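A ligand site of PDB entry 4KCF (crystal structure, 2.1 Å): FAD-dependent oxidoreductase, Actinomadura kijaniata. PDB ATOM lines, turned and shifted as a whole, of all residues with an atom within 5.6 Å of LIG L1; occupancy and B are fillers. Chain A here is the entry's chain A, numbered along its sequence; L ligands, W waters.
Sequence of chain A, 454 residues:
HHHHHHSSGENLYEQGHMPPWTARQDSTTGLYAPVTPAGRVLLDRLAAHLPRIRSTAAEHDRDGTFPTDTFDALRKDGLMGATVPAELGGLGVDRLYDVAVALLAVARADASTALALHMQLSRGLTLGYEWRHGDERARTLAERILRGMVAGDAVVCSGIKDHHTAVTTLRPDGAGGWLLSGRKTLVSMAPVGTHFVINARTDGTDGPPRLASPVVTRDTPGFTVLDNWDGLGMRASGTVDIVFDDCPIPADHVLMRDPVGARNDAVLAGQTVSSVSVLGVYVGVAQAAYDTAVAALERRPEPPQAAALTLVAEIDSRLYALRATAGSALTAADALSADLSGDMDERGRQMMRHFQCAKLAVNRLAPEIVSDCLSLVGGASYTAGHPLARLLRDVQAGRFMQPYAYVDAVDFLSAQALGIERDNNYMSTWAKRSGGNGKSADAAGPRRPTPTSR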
ATOM      1  N   LEU A 115      -9.248 -31.548 -23.016  1.00  0.00           N
ATOM      2  CA  LEU A 115     -10.427 -30.682 -23.016  1.00  0.00           C
ATOM      3  C   LEU A 115     -10.011 -29.202 -23.162  1.00  0.00           C
ATOM      4  O   LEU A 115     -10.575 -28.475 -23.985  1.00  0.00           O
ATOM      5  CB  LEU A 115     -11.261 -30.920 -21.743  1.00  0.00           C
ATOM      6  CG  LEU A 115     -12.434 -29.988 -21.387  1.00  0.00           C
ATOM      7  CD1 LEU A 115     -13.427 -30.009 -22.518  1.00  0.00           C
ATOM      8  CD2 LEU A 115     -13.146 -30.249 -20.028  1.00  0.00           C
ATOM      9  N   MET A 119     -10.424 -26.394 -26.600  1.00  0.00           N
ATOM     10  CA  MET A 119     -10.955 -25.025 -26.791  1.00  0.00           C
ATOM     11  C   MET A 119     -10.094 -24.197 -27.782  1.00  0.00           C
ATOM     12  O   MET A 119     -10.616 -23.491 -28.649  1.00  0.00           O
ATOM     13  CB  MET A 119     -11.121 -24.258 -25.474  1.00  0.00           C
ATOM     14  CG  MET A 119     -11.746 -25.005 -24.268  1.00  0.00           C
ATOM     15  SD  MET A 119     -13.421 -25.443 -24.723  1.00  0.00           S
ATOM     16  CE  MET A 119     -13.803 -26.417 -23.241  1.00  0.00           C
ATOM     17  N   SER A 158     -13.138 -19.627 -23.901  1.00  0.00           N
ATOM     18  CA  SER A 158     -14.483 -19.488 -24.448  1.00  0.00           C
ATOM     19  C   SER A 158     -15.410 -19.383 -23.248  1.00  0.00           C
ATOM     20  O   SER A 158     -15.332 -20.238 -22.354  1.00  0.00           O
ATOM     21  CB  SER A 158     -14.836 -20.715 -25.277  1.00  0.00           C
ATOM     22  OG  SER A 158     -16.255 -20.701 -25.441  1.00  0.00           O
ATOM     23  N   GLY A 159     -16.270 -18.364 -23.249  1.00  0.00           N
ATOM     24  CA  GLY A 159     -17.142 -18.066 -22.104  1.00  0.00           C
ATOM     25  C   GLY A 159     -18.591 -17.989 -22.564  1.00  0.00           C
ATOM     26  O   GLY A 159     -19.010 -16.917 -23.030  1.00  0.00           O
ATOM     27  N   ILE A 160     -19.356 -19.097 -22.471  1.00  0.00           N
ATOM     28  CA  ILE A 160     -20.708 -19.081 -23.031  1.00  0.00           C
ATOM     29  C   ILE A 160     -21.806 -18.937 -22.001  1.00  0.00           C
ATOM     30  O   ILE A 160     -22.744 -18.164 -22.175  1.00  0.00           O
ATOM     31  CB  ILE A 160     -21.057 -20.311 -23.932  1.00  0.00           C
ATOM     32  CG1 ILE A 160     -20.113 -20.415 -25.134  1.00  0.00           C
ATOM     33  CG2 ILE A 160     -22.558 -20.330 -24.277  1.00  0.00           C
ATOM     34  CD1 ILE A 160     -20.182 -19.369 -26.244  1.00  0.00           C
ATOM     35  N   LYS A 161     -21.707 -19.706 -20.929  1.00  0.00           N
ATOM     36  CA  LYS A 161     -22.800 -19.821 -19.955  1.00  0.00           C
ATOM     37  C   LYS A 161     -22.690 -18.800 -18.834  1.00  0.00           C
ATOM     38  O   LYS A 161     -21.686 -18.808 -18.096  1.00  0.00           O
ATOM     39  CB  LYS A 161     -22.762 -21.205 -19.280  1.00  0.00           C
ATOM     40  CG  LYS A 161     -23.892 -21.477 -18.288  1.00  0.00           C
ATOM     41  CD  LYS A 161     -23.831 -22.911 -17.787  1.00  0.00           C
ATOM     42  CE  LYS A 161     -25.219 -23.574 -17.891  1.00  0.00           C
ATOM     43  NZ  LYS A 161     -26.238 -22.812 -17.109  1.00  0.00           N
ATOM     44  N   THR A 185     -19.582 -18.720 -16.186  1.00  0.00           N
ATOM     45  CA  THR A 185     -19.098 -19.851 -15.413  1.00  0.00           C
ATOM     46  C   THR A 185     -18.527 -20.923 -16.340  1.00  0.00           C
ATOM     47  O   THR A 185     -18.880 -20.974 -17.523  1.00  0.00           O
ATOM     48  CB  THR A 185     -20.173 -20.373 -14.397  1.00  0.00           C
ATOM     49  OG1 THR A 185     -19.597 -21.415 -13.598  1.00  0.00           O
ATOM     50  CG2 THR A 185     -21.427 -20.846 -15.118  1.00  0.00           C
ATOM     51  N   LEU A 186     -17.617 -21.766 -15.856  1.00  0.00           N
ATOM     52  CA  LEU A 186     -17.078 -22.912 -16.623  1.00  0.00           C
ATOM     53  C   LEU A 186     -16.265 -22.428 -17.829  1.00  0.00           C
ATOM     54  O   LEU A 186     -16.717 -22.516 -18.974  1.00  0.00           O
ATOM     55  CB  LEU A 186     -18.204 -23.895 -17.021  1.00  0.00           C
ATOM     56  CG  LEU A 186     -19.091 -24.300 -15.828  1.00  0.00           C
ATOM     57  CD1 LEU A 186     -20.321 -25.077 -16.296  1.00  0.00           C
ATOM     58  CD2 LEU A 186     -18.310 -25.145 -14.825  1.00  0.00           C
ATOM     59  N   VAL A 187     -15.087 -21.843 -17.597  1.00  0.00           N
ATOM     60  CA  VAL A 187     -14.288 -21.321 -18.700  1.00  0.00           C
ATOM     61  C   VAL A 187     -12.979 -22.076 -18.632  1.00  0.00           C
ATOM     62  O   VAL A 187     -12.083 -21.658 -17.909  1.00  0.00           O
ATOM     63  CB  VAL A 187     -13.980 -19.801 -18.590  1.00  0.00           C
ATOM     64  CG1 VAL A 187     -13.267 -19.311 -19.853  1.00  0.00           C
ATOM     65  CG2 VAL A 187     -15.281 -18.980 -18.447  1.00  0.00           C
ATOM     66  N   SER A 188     -12.913 -23.221 -19.309  1.00  0.00           N
ATOM     67  CA  SER A 188     -11.721 -24.043 -19.224  1.00  0.00           C
ATOM     68  C   SER A 188     -10.548 -23.247 -19.815  1.00  0.00           C
ATOM     69  O   SER A 188     -10.776 -22.410 -20.706  1.00  0.00           O
ATOM     70  CB  SER A 188     -11.916 -25.325 -20.067  1.00  0.00           C
ATOM     71  OG  SER A 188     -13.091 -25.966 -19.590  1.00  0.00           O
ATOM     72  N   MET A 189      -9.358 -23.567 -19.315  1.00  0.00           N
ATOM     73  CA  MET A 189      -8.064 -23.033 -19.763  1.00  0.00           C
ATOM     74  C   MET A 189      -7.883 -21.595 -19.308  1.00  0.00           C
ATOM     75  O   MET A 189      -6.927 -20.941 -19.700  1.00  0.00           O
ATOM     76  CB  MET A 189      -7.866 -23.188 -21.271  1.00  0.00           C
ATOM     77  CG  MET A 189      -6.436 -22.987 -21.774  1.00  0.00           C
ATOM     78  SD  MET A 189      -6.292 -23.490 -23.503  1.00  0.00           S
ATOM     79  CE  MET A 189      -7.504 -22.501 -24.352  1.00  0.00           C
ATOM     80  N   TRP A 229     -12.519 -23.436  -9.423  1.00  0.00           N
ATOM     81  CA  TRP A 229     -12.918 -24.643 -10.186  1.00  0.00           C
ATOM     82  C   TRP A 229     -12.646 -25.771  -9.219  1.00  0.00           C
ATOM     83  O   TRP A 229     -11.487 -26.021  -8.930  1.00  0.00           O
ATOM     84  CB  TRP A 229     -12.065 -24.929 -11.448  1.00  0.00           C
ATOM     85  CG  TRP A 229     -12.376 -26.264 -12.146  1.00  0.00           C
ATOM     86  CD1 TRP A 229     -11.481 -27.153 -12.684  1.00  0.00           C
ATOM     87  CD2 TRP A 229     -13.691 -26.830 -12.390  1.00  0.00           C
ATOM     88  NE1 TRP A 229     -12.134 -28.244 -13.211  1.00  0.00           N
ATOM     89  CE2 TRP A 229     -13.485 -28.068 -13.057  1.00  0.00           C
ATOM     90  CE3 TRP A 229     -14.998 -26.446 -12.060  1.00  0.00           C
ATOM     91  CZ2 TRP A 229     -14.564 -28.894 -13.430  1.00  0.00           C
ATOM     92  CZ3 TRP A 229     -16.079 -27.251 -12.451  1.00  0.00           C
ATOM     93  CH2 TRP A 229     -15.846 -28.480 -13.122  1.00  0.00           C
ATOM     94  N   GLY A 233     -14.688 -34.407 -11.911  1.00  0.00           N
ATOM     95  CA  GLY A 233     -13.583 -34.724 -12.795  1.00  0.00           C
ATOM     96  C   GLY A 233     -13.158 -33.509 -13.616  1.00  0.00           C
ATOM     97  O   GLY A 233     -13.653 -32.395 -13.418  1.00  0.00           O
ATOM     98  N   MET A 234     -12.313 -33.750 -14.611  1.00  0.00           N
ATOM     99  CA  MET A 234     -11.742 -32.676 -15.436  1.00  0.00           C
ATOM    100  C   MET A 234     -11.170 -31.630 -14.438  1.00  0.00           C
ATOM    101  O   MET A 234     -11.293 -30.435 -14.638  1.00  0.00           O
ATOM    102  CB  MET A 234     -12.762 -32.030 -16.372  1.00  0.00           C
ATOM    103  CG  MET A 234     -13.319 -32.921 -17.486  1.00  0.00           C
ATOM    104  SD  MET A 234     -11.996 -33.725 -18.436  1.00  0.00           S
ATOM    105  CE  MET A 234     -12.937 -34.496 -19.777  1.00  0.00           C
ATOM    106  N   SER A 237      -8.661 -28.813 -15.630  1.00  0.00           N
ATOM    107  CA  SER A 237      -8.927 -28.160 -16.903  1.00  0.00           C
ATOM    108  C   SER A 237      -9.019 -26.648 -16.737  1.00  0.00           C
ATOM    109  O   SER A 237      -9.245 -25.961 -17.731  1.00  0.00           O
ATOM    110  CB  SER A 237     -10.211 -28.668 -17.593  1.00  0.00           C
ATOM    111  OG  SER A 237     -11.299 -28.377 -16.721  1.00  0.00           O
ATOM    112  N   THR A 239     -11.284 -24.725 -15.156  1.00  0.00           N
ATOM    113  CA  THR A 239     -12.643 -24.406 -15.596  1.00  0.00           C
ATOM    114  C   THR A 239     -13.334 -23.450 -14.600  1.00  0.00           C
ATOM    115  O   THR A 239     -14.406 -23.743 -14.044  1.00  0.00           O
ATOM    116  CB  THR A 239     -13.430 -25.740 -15.915  1.00  0.00           C
ATOM    117  OG1 THR A 239     -12.732 -26.425 -16.953  1.00  0.00           O
ATOM    118  CG2 THR A 239     -14.872 -25.520 -16.416  1.00  0.00           C
ATOM    119  N   ALA A 397     -17.846 -35.990 -17.960  1.00  0.00           N
ATOM    120  CA  ALA A 397     -17.956 -34.552 -18.269  1.00  0.00           C
ATOM    121  C   ALA A 397     -18.774 -34.184 -19.494  1.00  0.00           C
ATOM    122  O   ALA A 397     -19.458 -33.140 -19.517  1.00  0.00           O
ATOM    123  CB  ALA A 397     -16.540 -33.988 -18.367  1.00  0.00           C
ATOM    124  N   PHE A 400     -22.345 -33.077 -19.470  1.00  0.00           N
ATOM    125  CA  PHE A 400     -22.751 -31.749 -19.009  1.00  0.00           C
ATOM    126  C   PHE A 400     -22.282 -30.640 -19.953  1.00  0.00           C
ATOM    127  O   PHE A 400     -22.130 -29.497 -19.515  1.00  0.00           O
ATOM    128  CB  PHE A 400     -22.312 -31.537 -17.546  1.00  0.00           C
ATOM    129  CG  PHE A 400     -22.611 -32.763 -16.692  1.00  0.00           C
ATOM    130  CD1 PHE A 400     -23.918 -33.091 -16.395  1.00  0.00           C
ATOM    131  CD2 PHE A 400     -21.609 -33.616 -16.280  1.00  0.00           C
ATOM    132  CE1 PHE A 400     -24.224 -34.245 -15.675  1.00  0.00           C
ATOM    133  CE2 PHE A 400     -21.896 -34.793 -15.558  1.00  0.00           C
ATOM    134  CZ  PHE A 400     -23.222 -35.097 -15.263  1.00  0.00           C
ATOM    135  N   MET A 401     -21.991 -30.940 -21.206  1.00  0.00           N
ATOM    136  CA  MET A 401     -21.443 -29.903 -22.095  1.00  0.00           C
ATOM    137  C   MET A 401     -22.486 -29.612 -23.175  1.00  0.00           C
ATOM    138  O   MET A 401     -23.015 -30.513 -23.828  1.00  0.00           O
ATOM    139  CB  MET A 401     -20.137 -30.418 -22.704  1.00  0.00           C
ATOM    140  CG  MET A 401     -18.939 -30.306 -21.798  1.00  0.00           C
ATOM    141  SD  MET A 401     -17.488 -31.005 -22.598  1.00  0.00           S
ATOM    142  CE  MET A 401     -16.624 -30.801 -21.025  1.00  0.00           C
ATOM    143  N   GLN A 402     -22.829 -28.347 -23.344  1.00  0.00           N
ATOM    144  CA  GLN A 402     -23.792 -27.908 -24.372  1.00  0.00           C
ATOM    145  C   GLN A 402     -23.028 -27.519 -25.629  1.00  0.00           C
ATOM    146  O   GLN A 402     -21.921 -27.002 -25.500  1.00  0.00           O
ATOM    147  CB  GLN A 402     -24.487 -26.621 -23.911  1.00  0.00           C
ATOM    148  CG  GLN A 402     -25.328 -26.880 -22.662  1.00  0.00           C
ATOM    149  CD  GLN A 402     -26.683 -27.526 -22.996  1.00  0.00           C
ATOM    150  OE1 GLN A 402     -27.022 -27.732 -24.167  1.00  0.00           O
ATOM    151  NE2 GLN A 402     -27.458 -27.843 -21.960  1.00  0.00           N
ATOM    152  N   TRP A 430     -31.226 -19.443 -24.064  1.00  0.00           N
ATOM    153  CA  TRP A 430     -30.636 -18.963 -22.816  1.00  0.00           C
ATOM    154  C   TRP A 430     -30.815 -17.457 -22.654  1.00  0.00           C
ATOM    155  O   TRP A 430     -31.178 -16.999 -21.566  1.00  0.00           O
ATOM    156  CB  TRP A 430     -29.144 -19.323 -22.714  1.00  0.00           C
ATOM    157  CG  TRP A 430     -28.839 -20.758 -22.388  1.00  0.00           C
ATOM    158  CD1 TRP A 430     -29.741 -21.766 -22.119  1.00  0.00           C
ATOM    159  CD2 TRP A 430     -27.525 -21.349 -22.256  1.00  0.00           C
ATOM    160  NE1 TRP A 430     -29.065 -22.933 -21.842  1.00  0.00           N
ATOM    161  CE2 TRP A 430     -27.722 -22.710 -21.915  1.00  0.00           C
ATOM    162  CE3 TRP A 430     -26.226 -20.858 -22.401  1.00  0.00           C
ATOM    163  CZ2 TRP A 430     -26.637 -23.592 -21.708  1.00  0.00           C
ATOM    164  CZ3 TRP A 430     -25.153 -21.725 -22.195  1.00  0.00           C
ATOM    165  CH2 TRP A 430     -25.369 -23.077 -21.861  1.00  0.00           C
HETATM  166  N1  LIG L   1     -18.402 -23.947 -21.611  1.00  0.00           N
HETATM  167  C1  LIG L   1     -17.784 -22.965 -22.309  1.00  0.00           C
HETATM  168  O1  LIG L   1     -18.538 -22.151 -22.919  1.00  0.00           O
HETATM  169  N2  LIG L   1     -16.427 -22.897 -22.370  1.00  0.00           N
HETATM  170  C2  LIG L   1     -15.726 -23.793 -21.639  1.00  0.00           C
HETATM  171  O2  LIG L   1     -14.370 -23.747 -21.660  1.00  0.00           O
HETATM  172  C3  LIG L   1     -16.369 -24.846 -20.933  1.00  0.00           C
HETATM  173  N3  LIG L   1     -15.684 -25.796 -20.219  1.00  0.00           N
HETATM  174  C4  LIG L   1     -16.377 -26.721 -19.494  1.00  0.00           C
HETATM  175  C5  LIG L   1     -15.657 -27.680 -18.775  1.00  0.00           C
HETATM  176  C6  LIG L   1     -16.346 -28.664 -18.034  1.00  0.00           C
HETATM  177  C7  LIG L   1     -15.568 -29.687 -17.244  1.00  0.00           C
HETATM  178  C8  LIG L   1     -17.820 -28.691 -18.025  1.00  0.00           C
HETATM  179  C9  LIG L   1     -18.638 -29.713 -17.264  1.00  0.00           C
HETATM  180  C10 LIG L   1     -18.474 -27.720 -18.775  1.00  0.00           C
HETATM  181  C11 LIG L   1     -17.780 -26.744 -19.516  1.00  0.00           C
HETATM  182  N4  LIG L   1     -18.468 -25.795 -20.207  1.00  0.00           N
HETATM  183  C12 LIG L   1     -17.756 -24.893 -20.930  1.00  0.00           C
HETATM  184  C13 LIG L   1     -19.937 -25.641 -20.239  1.00  0.00           C
HETATM  185  C14 LIG L   1     -21.023 -26.653 -20.600  1.00  0.00           C
HETATM  186  O3  LIG L   1     -20.753 -26.611 -22.006  1.00  0.00           O
HETATM  187  C15 LIG L   1     -22.515 -26.488 -20.191  1.00  0.00           C
HETATM  188  O4  LIG L   1     -23.088 -25.188 -20.481  1.00  0.00           O
HETATM  189  C16 LIG L   1     -23.068 -26.794 -18.768  1.00  0.00           C
HETATM  190  O5  LIG L   1     -22.354 -27.577 -17.769  1.00  0.00           O
HETATM  191  O1  LG2 L   2     -20.206 -22.401 -31.021  1.00  0.00           O
HETATM  192  P1  LG2 L   2     -20.255 -20.974 -31.566  1.00  0.00           P
HETATM  193  O2  LG2 L   2     -21.580 -20.266 -31.588  1.00  0.00           O
HETATM  194  O3  LG2 L   2     -19.292 -20.039 -30.710  1.00  0.00           O
HETATM  195  P2  LG2 L   2     -17.827 -20.351 -30.145  1.00  0.00           P
HETATM  196  O4  LG2 L   2     -17.264 -18.968 -29.841  1.00  0.00           O
HETATM  197  O5  LG2 L   2     -18.084 -21.064 -28.737  1.00  0.00           O
HETATM  198  C1  LG2 L   2     -17.881 -22.444 -28.461  1.00  0.00           C
HETATM  199  C2  LG2 L   2     -18.625 -22.841 -27.183  1.00  0.00           C
HETATM  200  C3  LG2 L   2     -18.101 -24.185 -26.672  1.00  0.00           C
HETATM  201  C4  LG2 L   2     -18.823 -25.189 -27.583  1.00  0.00           C
HETATM  202  N1  LG2 L   2     -18.521 -24.426 -25.281  1.00  0.00           N
HETATM  203  C5  LG2 L   2     -16.570 -24.274 -26.629  1.00  0.00           C
HETATM  204  O6  LG2 L   2     -16.056 -23.717 -25.408  1.00  0.00           O
HETATM  205  O7  LG2 L   2     -16.164 -25.654 -26.576  1.00  0.00           O
HETATM  206  C6  LG2 L   2     -15.774 -23.336 -27.532  1.00  0.00           C
HETATM  207  C7  LG2 L   2     -14.456 -23.791 -28.160  1.00  0.00           C
HETATM  208  O8  LG2 L   2     -16.458 -22.481 -28.438  1.00  0.00           O
HETATM  209  O9  LG2 L   2     -16.952 -21.259 -30.980  1.00  0.00           O
HETATM  210  O10 LG2 L   2     -19.688 -21.038 -33.069  1.00  0.00           O
HETATM  211  C8  LG2 L   2     -19.690 -19.811 -33.807  1.00  0.00           C
HETATM  212  C9  LG2 L   2     -18.473 -19.949 -34.705  1.00  0.00           C
HETATM  213  C10 LG2 L   2     -18.165 -18.686 -35.516  1.00  0.00           C
HETATM  214  O11 LG2 L   2     -17.125 -17.977 -34.844  1.00  0.00           O
HETATM  215  C11 LG2 L   2     -17.648 -19.173 -36.853  1.00  0.00           C
HETATM  216  C12 LG2 L   2     -17.936 -20.680 -36.873  1.00  0.00           C
HETATM  217  O12 LG2 L   2     -18.720 -20.952 -35.693  1.00  0.00           O
HETATM  218  N2  LG2 L   2     -18.644 -21.196 -38.046  1.00  0.00           N
HETATM  219  C13 LG2 L   2     -18.086 -22.191 -38.733  1.00  0.00           C
HETATM  220  O13 LG2 L   2     -16.863 -22.654 -38.376  1.00  0.00           O
HETATM  221  N3  LG2 L   2     -18.665 -22.749 -39.810  1.00  0.00           N
HETATM  222  C14 LG2 L   2     -19.882 -22.311 -40.185  1.00  0.00           C
HETATM  223  O14 LG2 L   2     -20.526 -22.842 -41.253  1.00  0.00           O
HETATM  224  C15 LG2 L   2     -20.559 -21.237 -39.427  1.00  0.00           C
HETATM  225  C16 LG2 L   2     -21.922 -20.766 -39.851  1.00  0.00           C
HETATM  226  C17 LG2 L   2     -19.862 -20.714 -38.356  1.00  0.00           C
HETATM  227  O   HOH W   1     -12.335 -22.178 -22.763  1.00  0.00           O
HETATM  228  O   HOH W   2     -19.111 -21.054 -20.127  1.00  0.00           O
HETATM  229  O   HOH W   3     -18.268 -26.827 -23.739  1.00  0.00           O
HETATM  230  O   HOH W   4     -21.426 -23.494 -22.507  1.00  0.00           O
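Water W1 lies within hydrogen-bond range of the backbone carbonyl oxygen of Ser 188 (2.6 Å), an oxygen (O2) of LIG L1 (2.8 Å) and the backbone NH of Ser 158 (2.9 Å).
Water W3 lies within hydrogen-bond range of a nitrogen (N1) of LG2 L2 and an oxygen (O3) of LIG L1.
NE1 of Trp 229 sits at hydrogen-bond distance from O of Met 234, 2.7 Å away.
The backbone carbonyl oxygen (O) of Met 234 lies within hydrogen-bond range of the side-chain hydroxyl (OG) of Ser 237 (2.9 Å).
The backbone carbonyl oxygen (O) of Lys 161 lies within hydrogen-bond range of the backbone NH (N) of Thr 185.
OG of Ser 188 lies within hydrogen-bond range of OG1 of Thr 239.
The side-chain hydroxyl of Ser 237 lies within hydrogen-bond range of the side-chain hydroxyl of Thr 239, 2.4 Å away.
A nitrogen (N2) of LIG L1 is in hydrogen-bond range of an oxygen (O6) of LG2 L2.
An oxygen (O2) of LIG L1 lies close to the side-chain sulfur of Met 119 (3.6 Å).
CD2 of Leu 115 touches C7 of LIG L1, 3.7 Å away.
Lys 161 touches LIG L1 (CD to O4, 3.6 Å).
C of Val 187 touches O2 of LIG L1, 3.7 Å away.
Met 234 touches LIG L1.
Thr 239 touches LIG L1 (CG2 to C5, 3.3 Å).
Met 401 touches LIG L1 (CA to O3, 3.4 Å).
Trp 430 touches LIG L1 (CH2 to O4, 3.4 Å).
Within 4 Å of LIG L1: Leu 115, Met 119, Ser 158, Ile 160, Lys 161, Leu 186, Val 187, Ser 188, Met 234, Thr 239, Phe 400, Met 401, Gln 402 and Trp 430.
The nearest printed residue that does not touch LIG L1 is Trp 229 (4.02 Å).
The side-chain sulfur (SD) of Met 119 sits at hydrogen-bond distance from an oxygen (O6) of LG2 L2, at 3.2 Å.
N of Gln 402 is in hydrogen-bond range of O3 of LIG L1, at 3.0 Å.
An oxygen (O2) of LIG L1 is in hydrogen-bond range of the backbone NH (N) of Ser 188, at 2.8 Å.
The backbone NH of Ile 160 sits at hydrogen-bond distance from an oxygen (O1) of LIG L1 (3.2 Å).
O of Phe 400 is in hydrogen-bond range of O5 of LIG L1 (2.6 Å).
An oxygen (O6) of LG2 L2 sits at hydrogen-bond distance from the side-chain hydroxyl of Ser 158, at 3.0 Å.
A nitrogen (N2) of LIG L1 lies close to the backbone carbonyl oxygen (O) of Leu 186 (3.4 Å).
A nitrogen (N3) of LIG L1 is in hydrogen-bond range of the side-chain hydroxyl (OG) of Ser 188.
The backbone carbonyl oxygen (O) of Ser 158 lies within hydrogen-bond range of a nitrogen (N2) of LIG L1 (2.9 Å).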
